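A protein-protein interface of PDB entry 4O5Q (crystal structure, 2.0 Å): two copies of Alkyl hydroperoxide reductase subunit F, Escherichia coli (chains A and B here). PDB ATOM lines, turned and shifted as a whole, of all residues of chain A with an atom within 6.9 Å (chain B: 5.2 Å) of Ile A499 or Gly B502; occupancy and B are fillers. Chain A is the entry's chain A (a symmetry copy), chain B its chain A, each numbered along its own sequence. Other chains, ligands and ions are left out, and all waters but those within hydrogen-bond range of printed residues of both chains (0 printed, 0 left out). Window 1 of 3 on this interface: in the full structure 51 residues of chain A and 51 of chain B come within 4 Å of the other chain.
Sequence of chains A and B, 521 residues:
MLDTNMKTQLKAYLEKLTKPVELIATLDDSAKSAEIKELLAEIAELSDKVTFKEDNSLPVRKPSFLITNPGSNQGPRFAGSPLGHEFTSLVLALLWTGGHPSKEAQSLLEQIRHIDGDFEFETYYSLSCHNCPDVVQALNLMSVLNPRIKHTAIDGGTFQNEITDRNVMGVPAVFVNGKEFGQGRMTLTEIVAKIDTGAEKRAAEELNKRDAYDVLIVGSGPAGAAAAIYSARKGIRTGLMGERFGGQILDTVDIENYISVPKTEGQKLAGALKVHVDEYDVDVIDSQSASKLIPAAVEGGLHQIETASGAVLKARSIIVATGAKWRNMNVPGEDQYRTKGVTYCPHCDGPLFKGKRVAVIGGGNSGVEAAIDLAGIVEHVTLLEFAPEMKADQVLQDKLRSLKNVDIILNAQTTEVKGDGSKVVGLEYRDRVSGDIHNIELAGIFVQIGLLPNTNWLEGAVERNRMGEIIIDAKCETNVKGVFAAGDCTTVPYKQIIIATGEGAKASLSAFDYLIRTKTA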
ATOM      1  N   ALA A 223     -18.612  25.299   1.950  1.00  0.00           N
ATOM      2  CA  ALA A 223     -17.397  24.561   1.580  1.00  0.00           C
ATOM      3  C   ALA A 223     -16.259  24.800   2.576  1.00  0.00           C
ATOM      4  O   ALA A 223     -15.584  23.869   3.020  1.00  0.00           O
ATOM      5  CB  ALA A 223     -16.942  24.906   0.166  1.00  0.00           C
ATOM      6  N   TYR A 258     -31.062  20.575   1.567  1.00  0.00           N
ATOM      7  CA  TYR A 258     -29.900  20.167   2.346  1.00  0.00           C
ATOM      8  C   TYR A 258     -30.203  18.761   2.882  1.00  0.00           C
ATOM      9  O   TYR A 258     -30.959  18.597   3.834  1.00  0.00           O
ATOM     10  CB  TYR A 258     -29.496  21.144   3.483  1.00  0.00           C
ATOM     11  CG  TYR A 258     -28.115  20.820   3.993  1.00  0.00           C
ATOM     12  CD1 TYR A 258     -26.991  21.185   3.264  1.00  0.00           C
ATOM     13  CD2 TYR A 258     -27.922  20.094   5.158  1.00  0.00           C
ATOM     14  CE1 TYR A 258     -25.743  20.899   3.678  1.00  0.00           C
ATOM     15  CE2 TYR A 258     -26.635  19.786   5.587  1.00  0.00           C
ATOM     16  CZ  TYR A 258     -25.561  20.181   4.855  1.00  0.00           C
ATOM     17  OH  TYR A 258     -24.293  19.912   5.250  1.00  0.00           O
ATOM     18  N   ILE A 259     -29.637  17.767   2.206  1.00  0.00           N
ATOM     19  CA  ILE A 259     -30.041  16.392   2.364  1.00  0.00           C
ATOM     20  C   ILE A 259     -30.066  15.957   3.837  1.00  0.00           C
ATOM     21  O   ILE A 259     -29.115  16.140   4.582  1.00  0.00           O
ATOM     22  CB  ILE A 259     -29.142  15.450   1.495  1.00  0.00           C
ATOM     23  CG1 ILE A 259     -29.198  15.870   0.012  1.00  0.00           C
ATOM     24  CG2 ILE A 259     -29.522  13.987   1.707  1.00  0.00           C
ATOM     25  CD1 ILE A 259     -30.584  15.965  -0.612  1.00  0.00           C
ATOM     26  N   GLY A 487     -16.012  23.937  -3.700  1.00  0.00           N
ATOM     27  CA  GLY A 487     -17.234  24.692  -3.735  1.00  0.00           C
ATOM     28  C   GLY A 487     -17.435  25.484  -5.015  1.00  0.00           C
ATOM     29  O   GLY A 487     -16.822  25.217  -6.084  1.00  0.00           O
ATOM     30  N   ASP A 488     -18.347  26.452  -4.923  1.00  0.00           N
ATOM     31  CA  ASP A 488     -18.787  27.146  -6.121  1.00  0.00           C
ATOM     32  C   ASP A 488     -17.674  27.873  -6.880  1.00  0.00           C
ATOM     33  O   ASP A 488     -17.835  28.148  -8.059  1.00  0.00           O
ATOM     34  CB  ASP A 488     -19.892  28.169  -5.763  1.00  0.00           C
ATOM     35  CG  ASP A 488     -21.201  27.517  -5.432  1.00  0.00           C
ATOM     36  OD1 ASP A 488     -21.279  26.267  -5.391  1.00  0.00           O
ATOM     37  OD2 ASP A 488     -22.152  28.265  -5.184  1.00  0.00           O
ATOM     38  N   VAL A 492     -16.382  22.604 -10.190  1.00  0.00           N
ATOM     39  CA  VAL A 492     -17.500  21.732  -9.831  1.00  0.00           C
ATOM     40  C   VAL A 492     -18.747  22.133 -10.647  1.00  0.00           C
ATOM     41  O   VAL A 492     -19.094  23.312 -10.735  1.00  0.00           O
ATOM     42  CB  VAL A 492     -17.734  21.684  -8.312  1.00  0.00           C
ATOM     43  CG1 VAL A 492     -18.346  22.994  -7.777  1.00  0.00           C
ATOM     44  CG2 VAL A 492     -18.660  20.522  -7.956  1.00  0.00           C
ATOM     45  N   PRO A 493     -19.405  21.152 -11.307  1.00  0.00           N
ATOM     46  CA  PRO A 493     -20.370  21.567 -12.340  1.00  0.00           C
ATOM     47  C   PRO A 493     -21.696  22.099 -11.859  1.00  0.00           C
ATOM     48  O   PRO A 493     -22.353  22.753 -12.646  1.00  0.00           O
ATOM     49  CB  PRO A 493     -20.568  20.304 -13.183  1.00  0.00           C
ATOM     50  CG  PRO A 493     -20.197  19.165 -12.275  1.00  0.00           C
ATOM     51  CD  PRO A 493     -19.048  19.732 -11.435  1.00  0.00           C
ATOM     52  N   TYR A 494     -22.080  21.845 -10.610  1.00  0.00           N
ATOM     53  CA  TYR A 494     -23.325  22.356 -10.069  1.00  0.00           C
ATOM     54  C   TYR A 494     -23.008  23.073  -8.758  1.00  0.00           C
ATOM     55  O   TYR A 494     -22.006  22.768  -8.105  1.00  0.00           O
ATOM     56  CB  TYR A 494     -24.313  21.194  -9.895  1.00  0.00           C
ATOM     57  CG  TYR A 494     -24.418  20.351 -11.153  1.00  0.00           C
ATOM     58  CD1 TYR A 494     -25.026  20.850 -12.304  1.00  0.00           C
ATOM     59  CD2 TYR A 494     -23.893  19.071 -11.187  1.00  0.00           C
ATOM     60  CE1 TYR A 494     -25.113  20.080 -13.456  1.00  0.00           C
ATOM     61  CE2 TYR A 494     -23.978  18.304 -12.308  1.00  0.00           C
ATOM     62  CZ  TYR A 494     -24.568  18.820 -13.445  1.00  0.00           C
ATOM     63  OH  TYR A 494     -24.603  18.020 -14.545  1.00  0.00           O
ATOM     64  N   LYS A 495     -23.845  24.039  -8.403  1.00  0.00           N
ATOM     65  CA  LYS A 495     -23.577  25.010  -7.322  1.00  0.00           C
ATOM     66  C   LYS A 495     -24.724  24.850  -6.355  1.00  0.00           C
ATOM     67  O   LYS A 495     -25.820  25.377  -6.581  1.00  0.00           O
ATOM     68  CB  LYS A 495     -23.539  26.463  -7.864  1.00  0.00           C
ATOM     69  CG  LYS A 495     -22.696  26.590  -9.154  1.00  0.00           C
ATOM     70  CD  LYS A 495     -21.206  26.225  -8.951  1.00  0.00           C
ATOM     71  CE  LYS A 495     -20.445  26.291 -10.286  1.00  0.00           C
ATOM     72  NZ  LYS A 495     -18.968  26.196 -10.091  1.00  0.00           N
ATOM     73  N   GLN A 496     -24.505  24.023  -5.331  1.00  0.00           N
ATOM     74  CA  GLN A 496     -25.522  23.774  -4.326  1.00  0.00           C
ATOM     75  C   GLN A 496     -24.817  23.639  -2.987  1.00  0.00           C
ATOM     76  O   GLN A 496     -23.638  23.324  -2.947  1.00  0.00           O
ATOM     77  CB  GLN A 496     -26.260  22.469  -4.628  1.00  0.00           C
ATOM     78  CG  GLN A 496     -27.135  22.493  -5.880  1.00  0.00           C
ATOM     79  CD  GLN A 496     -28.441  23.217  -5.647  1.00  0.00           C
ATOM     80  OE1 GLN A 496     -29.422  22.614  -5.213  1.00  0.00           O
ATOM     81  NE2 GLN A 496     -28.474  24.518  -5.958  1.00  0.00           N
ATOM     82  N   ILE A 497     -25.561  23.782  -1.901  1.00  0.00           N
ATOM     83  CA  ILE A 497     -24.975  23.693  -0.579  1.00  0.00           C
ATOM     84  C   ILE A 497     -24.420  22.292  -0.320  1.00  0.00           C
ATOM     85  O   ILE A 497     -23.276  22.160   0.090  1.00  0.00           O
ATOM     86  CB  ILE A 497     -25.993  24.030   0.535  1.00  0.00           C
ATOM     87  CG1 ILE A 497     -26.595  25.422   0.326  1.00  0.00           C
ATOM     88  CG2 ILE A 497     -25.312  23.961   1.926  1.00  0.00           C
ATOM     89  CD1 ILE A 497     -27.930  25.630   1.081  1.00  0.00           C
ATOM     90  N   ILE A 498     -25.213  21.267  -0.600  1.00  0.00           N
ATOM     91  CA  ILE A 498     -24.833  19.920  -0.216  1.00  0.00           C
ATOM     92  C   ILE A 498     -23.630  19.520  -1.079  1.00  0.00           C
ATOM     93  O   ILE A 498     -22.778  18.803  -0.644  1.00  0.00           O
ATOM     94  CB  ILE A 498     -25.996  18.890  -0.348  1.00  0.00           C
ATOM     95  CG1 ILE A 498     -25.582  17.539   0.300  1.00  0.00           C
ATOM     96  CG2 ILE A 498     -26.376  18.611  -1.762  1.00  0.00           C
ATOM     97  CD1 ILE A 498     -25.597  17.621   1.788  1.00  0.00           C
ATOM     98  N   ILE A 499     -23.549  20.051  -2.295  1.00  0.00           N
ATOM     99  CA  ILE A 499     -22.417  19.770  -3.171  1.00  0.00           C
ATOM    100  C   ILE A 499     -21.151  20.438  -2.635  1.00  0.00           C
ATOM    101  O   ILE A 499     -20.088  19.806  -2.528  1.00  0.00           O
ATOM    102  CB  ILE A 499     -22.741  20.184  -4.604  1.00  0.00           C
ATOM    103  CG1 ILE A 499     -23.931  19.318  -5.102  1.00  0.00           C
ATOM    104  CG2 ILE A 499     -21.486  20.067  -5.534  1.00  0.00           C
ATOM    105  CD1 ILE A 499     -24.420  19.669  -6.504  1.00  0.00           C
ATOM    106  N   ALA A 500     -21.277  21.709  -2.282  1.00  0.00           N
ATOM    107  CA  ALA A 500     -20.179  22.485  -1.734  1.00  0.00           C
ATOM    108  C   ALA A 500     -19.634  21.845  -0.454  1.00  0.00           C
ATOM    109  O   ALA A 500     -18.435  21.787  -0.285  1.00  0.00           O
ATOM    110  CB  ALA A 500     -20.612  23.963  -1.486  1.00  0.00           C
ATOM    111  N   THR A 501     -20.487  21.356   0.430  1.00  0.00           N
ATOM    112  CA  THR A 501     -19.990  20.808   1.691  1.00  0.00           C
ATOM    113  C   THR A 501     -19.211  19.532   1.425  1.00  0.00           C
ATOM    114  O   THR A 501     -18.168  19.312   2.026  1.00  0.00           O
ATOM    115  CB  THR A 501     -21.137  20.508   2.730  1.00  0.00           C
ATOM    116  OG1 THR A 501     -22.158  19.721   2.085  1.00  0.00           O
ATOM    117  CG2 THR A 501     -21.749  21.796   3.175  1.00  0.00           C
ATOM    118  N   GLY A 502     -19.739  18.687   0.546  1.00  0.00           N
ATOM    119  CA  GLY A 502     -19.017  17.504   0.108  1.00  0.00           C
ATOM    120  C   GLY A 502     -17.615  17.828  -0.430  1.00  0.00           C
ATOM    121  O   GLY A 502     -16.635  17.161  -0.136  1.00  0.00           O
ATOM    122  N   GLU A 503     -17.531  18.856  -1.269  1.00  0.00           N
ATOM    123  CA  GLU A 503     -16.271  19.247  -1.860  1.00  0.00           C
ATOM    124  C   GLU A 503     -15.307  19.742  -0.809  1.00  0.00           C
ATOM    125  O   GLU A 503     -14.096  19.465  -0.885  1.00  0.00           O
ATOM    126  CB  GLU A 503     -16.456  20.362  -2.948  1.00  0.00           C
ATOM    127  CG  GLU A 503     -17.314  19.911  -4.126  1.00  0.00           C
ATOM    128  CD  GLU A 503     -16.595  18.893  -5.023  1.00  0.00           C
ATOM    129  OE1 GLU A 503     -15.464  19.220  -5.460  1.00  0.00           O
ATOM    130  OE2 GLU A 503     -17.180  17.815  -5.343  1.00  0.00           O
ATOM    131  N   GLY A 504     -15.804  20.484   0.161  1.00  0.00           N
ATOM    132  CA  GLY A 504     -14.927  20.990   1.224  1.00  0.00           C
ATOM    133  C   GLY A 504     -14.291  19.859   2.029  1.00  0.00           C
ATOM    134  O   GLY A 504     -13.115  19.898   2.370  1.00  0.00           O
ATOM    135  N   LYS A 506     -13.731  16.802   0.850  1.00  0.00           N
ATOM    136  CA  LYS A 506     -12.718  16.231  -0.022  1.00  0.00           C
ATOM    137  C   LYS A 506     -11.425  17.057  -0.027  1.00  0.00           C
ATOM    138  O   LYS A 506     -10.343  16.497   0.033  1.00  0.00           O
ATOM    139  CB  LYS A 506     -13.197  16.069  -1.446  1.00  0.00           C
ATOM    140  CG  LYS A 506     -14.312  15.061  -1.611  1.00  0.00           C
ATOM    141  CD  LYS A 506     -14.580  14.690  -3.099  1.00  0.00           C
ATOM    142  CE  LYS A 506     -15.326  15.779  -3.829  1.00  0.00           C
ATOM    143  NZ  LYS A 506     -15.821  15.306  -5.154  1.00  0.00           N
ATOM    144  N   ILE B 497     -19.997  10.150   4.362  1.00  0.00           N
ATOM    145  CA  ILE B 497     -21.406  10.409   4.140  1.00  0.00           C
ATOM    146  C   ILE B 497     -21.609  11.738   3.410  1.00  0.00           C
ATOM    147  O   ILE B 497     -22.314  11.779   2.412  1.00  0.00           O
ATOM    148  CB  ILE B 497     -22.208  10.448   5.461  1.00  0.00           C
ATOM    149  CG1 ILE B 497     -22.037   9.144   6.246  1.00  0.00           C
ATOM    150  CG2 ILE B 497     -23.713  10.687   5.170  1.00  0.00           C
ATOM    151  CD1 ILE B 497     -22.388   9.285   7.747  1.00  0.00           C
ATOM    152  N   ILE B 498     -20.962  12.793   3.886  1.00  0.00           N
ATOM    153  CA  ILE B 498     -21.240  14.119   3.365  1.00  0.00           C
ATOM    154  C   ILE B 498     -20.720  14.163   1.923  1.00  0.00           C
ATOM    155  O   ILE B 498     -21.276  14.819   1.094  1.00  0.00           O
ATOM    156  CB  ILE B 498     -20.624  15.261   4.229  1.00  0.00           C
ATOM    157  CG1 ILE B 498     -21.160  16.637   3.745  1.00  0.00           C
ATOM    158  CG2 ILE B 498     -19.136  15.311   4.160  1.00  0.00           C
ATOM    159  CD1 ILE B 498     -22.573  16.851   4.167  1.00  0.00           C
ATOM    160  N   ILE B 499     -19.672  13.399   1.630  1.00  0.00           N
ATOM    161  CA  ILE B 499     -19.136  13.336   0.275  1.00  0.00           C
ATOM    162  C   ILE B 499     -20.112  12.608  -0.649  1.00  0.00           C
ATOM    163  O   ILE B 499     -20.433  13.087  -1.748  1.00  0.00           O
ATOM    164  CB  ILE B 499     -17.747  12.702   0.284  1.00  0.00           C
ATOM    165  CG1 ILE B 499     -16.802  13.619   1.108  1.00  0.00           C
ATOM    166  CG2 ILE B 499     -17.221  12.451  -1.170  1.00  0.00           C
ATOM    167  CD1 ILE B 499     -15.385  13.076   1.269  1.00  0.00           C
ATOM    168  N   ALA B 500     -20.593  11.462  -0.190  1.00  0.00           N
ATOM    169  CA  ALA B 500     -21.547  10.656  -0.931  1.00  0.00           C
ATOM    170  C   ALA B 500     -22.823  11.447  -1.234  1.00  0.00           C
ATOM    171  O   ALA B 500     -23.326  11.362  -2.333  1.00  0.00           O
ATOM    172  CB  ALA B 500     -21.869   9.335  -0.169  1.00  0.00           C
ATOM    173  N   THR B 501     -23.336  12.218  -0.290  1.00  0.00           N
ATOM    174  CA  THR B 501     -24.593  12.924  -0.534  1.00  0.00           C
ATOM    175  C   THR B 501     -24.385  13.995  -1.589  1.00  0.00           C
ATOM    176  O   THR B 501     -25.227  14.174  -2.459  1.00  0.00           O
ATOM    177  CB  THR B 501     -25.194  13.584   0.764  1.00  0.00           C
ATOM    178  OG1 THR B 501     -24.171  14.371   1.406  1.00  0.00           O
ATOM    179  CG2 THR B 501     -25.623  12.511   1.712  1.00  0.00           C
ATOM    180  N   GLY B 502     -23.277  14.720  -1.486  1.00  0.00           N
ATOM    181  CA  GLY B 502     -22.902  15.678  -2.515  1.00  0.00           C
ATOM    182  C   GLY B 502     -22.852  15.053  -3.917  1.00  0.00           C
ATOM    183  O   GLY B 502     -23.320  15.615  -4.896  1.00  0.00           O
ATOM    184  N   GLU B 503     -22.234  13.881  -4.018  1.00  0.00           N
ATOM    185  CA  GLU B 503     -22.103  13.203  -5.287  1.00  0.00           C
ATOM    186  C   GLU B 503     -23.452  12.786  -5.825  1.00  0.00           C
ATOM    187  O   GLU B 503     -23.695  12.864  -7.043  1.00  0.00           O
ATOM    188  CB  GLU B 503     -21.183  11.936  -5.183  1.00  0.00           C
ATOM    189  CG  GLU B 503     -19.753  12.269  -4.770  1.00  0.00           C
ATOM    190  CD  GLU B 503     -18.968  12.976  -5.884  1.00  0.00           C
ATOM    191  OE1 GLU B 503     -18.935  12.409  -7.004  1.00  0.00           O
ATOM    192  OE2 GLU B 503     -18.337  14.045  -5.626  1.00  0.00           O
ATOM    193  N   GLY B 504     -24.330  12.329  -4.955  1.00  0.00           N
ATOM    194  CA  GLY B 504     -25.666  11.917  -5.405  1.00  0.00           C
ATOM    195  C   GLY B 504     -26.448  13.079  -6.014  1.00  0.00           C
ATOM    196  O   GLY B 504     -27.121  12.936  -7.028  1.00  0.00           O
ATOM    197  N   ALA B 505     -26.345  14.241  -5.395  1.00  0.00           N
ATOM    198  CA  ALA B 505     -26.944  15.456  -5.943  1.00  0.00           C
ATOM    199  C   ALA B 505     -26.372  15.790  -7.308  1.00  0.00           C
ATOM    200  O   ALA B 505     -27.138  16.101  -8.236  1.00  0.00           O
ATOM    201  CB  ALA B 505     -26.725  16.649  -4.993  1.00  0.00           C
ATOM    202  N   LYS B 506     -25.053  15.732  -7.450  1.00  0.00           N
ATOM    203  CA  LYS B 506     -24.443  15.969  -8.748  1.00  0.00           C
ATOM    204  C   LYS B 506     -24.938  14.977  -9.810  1.00  0.00           C
ATOM    205  O   LYS B 506     -25.231  15.374 -10.925  1.00  0.00           O
ATOM    206  CB  LYS B 506     -22.933  15.918  -8.702  1.00  0.00           C
ATOM    207  CG  LYS B 506     -22.303  17.026  -7.889  1.00  0.00           C
ATOM    208  CD  LYS B 506     -20.765  17.134  -8.100  1.00  0.00           C
ATOM    209  CE  LYS B 506     -20.015  16.045  -7.375  1.00  0.00           C
ATOM    210  NZ  LYS B 506     -18.549  16.317  -7.349  1.00  0.00           N
ATOM    211  N   LEU B 509     -28.401  15.816 -10.983  1.00  0.00           N
ATOM    212  CA  LEU B 509     -28.476  16.967 -11.884  1.00  0.00           C
ATOM    213  C   LEU B 509     -27.925  16.616 -13.243  1.00  0.00           C
ATOM    214  O   LEU B 509     -28.427  17.093 -14.258  1.00  0.00           O
ATOM    215  CB  LEU B 509     -27.757  18.170 -11.269  1.00  0.00           C
ATOM    216  CG  LEU B 509     -28.471  18.686 -10.010  1.00  0.00           C
ATOM    217  CD1 LEU B 509     -27.597  19.743  -9.267  1.00  0.00           C
ATOM    218  CD2 LEU B 509     -29.866  19.263 -10.316  1.00  0.00           C
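The side-chain amino group of Lys A506 is in salt-bridge range of the side-chain carboxylate of Glu B503, at 2.9 Å. The side-chain amino group (NZ) of Lys B506 lies within salt-bridge range of the side-chain carboxylate (OE2) of Glu A503 (2.9 Å).
O of Ile B497 sits at hydrogen-bond distance from OG1 of Thr B501 (3.3 Å). The side-chain carboxylate (OE2) of Glu B503 is in salt-bridge range of the side-chain amino group (NZ) of Lys B506. O of Val A492 lies within hydrogen-bond range of NZ of Lys A495 (3.0 Å). The side-chain hydroxyl of Thr A501 lies within hydrogen-bond range of the backbone carbonyl oxygen of Ile A497 (3.3 Å). O of Ile A498 is in hydrogen-bond range of OG1 of Thr A501 (2.9 Å). The side-chain amino group of Lys A506 is in salt-bridge range of the side-chain carboxylate of Glu A503, 2.9 Å away.
Among the printed residues, pairs that only touch across the chains: Tyr A258 with Ile B498 (3.7 Å), Val A492 with Lys B506 (3.99 Å), Tyr A494 with Lys B506 (3.5 Å), Tyr A494 with Leu B509 (3.6 Å), Ile A498 with Ile B498 (3.9 Å), Ile A498 with Thr B501 (3.6 Å), Ile A498 with Gly B502 (3.6 Å), Ile A498 with Ala B505 (3.8 Å), Ile A499 with Gly B502 (3.8 Å), Ile A499 with Ala B505 (3.9 Å), Ile A499 with Lys B506 (3.7 Å), Thr A501 with Ile B498 (3.6 Å), Gly A502 with Ile B498 (3.6 Å), Gly A502 with Ile B499 (3.8 Å), Glu A503 with Glu B503 (3.95 Å), Lys A506 with Ile B499 (3.7 Å) and Lys A506 with Lys B506 (3.6 Å).
Ile A499 touches just these residues of chain B: Gly B502, Ala B505 and Lys B506. Gly B502 touches two residues of chain A. Printed residues of chain B within 4 Å of Tyr A258: Ile B498 (3.7 Å). Of the printed residues of chain B, Val A492 touches Lys B506 (3.99 Å). Of the printed residues of chain A, Ala B505 touches Ile A498 and Ile A499. Of the printed residues of chain B, Thr A501 touches Ile B498. Lys A495 touches none of the printed residues of chain B. The nearest residue of chain B that does not touch Ile A499 is Leu B509 (4.2 Å). The nearest printed residue of chain A that does not touch Leu B509 is Ile A499 (4.2 Å).
Hydrophobic or aromatic side chains of chain B within 4 Å of the printed part of chain A: Ile B498, Ile B499, Ala B505 and Leu B509. Of the 19 printed residues of chain A, 9 touch a printed residue of chain B. Printed residues of chain A that touch a printed residue of chain B: Tyr A258, Val A492, Tyr A494, Ile A498, Ile A499, Thr A501, Gly A502, Glu A503 and Lys A506. Among the printed residues, 19 pairs touch across the chains. Among the printed residues, Asp or Glu carboxylates within 4 Å of a Lys or Arg side-chain nitrogen of the other chain: Glu A503 with Lys B506 and Lys A506 with Glu B503.
Ile A498 touches Thr B501, and with the chains exchanged Thr A501 touches Ile B498. Ile A498 touches Gly B502, and with the chains exchanged Gly A502 touches Ile B498. Ile A499 touches Lys B506, and with the chains exchanged Lys A506 touches Ile B499. Glu A503 touches Lys B506, and with the chains exchanged Lys A506 touches Glu B503. 9 positions are printed for both chains.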
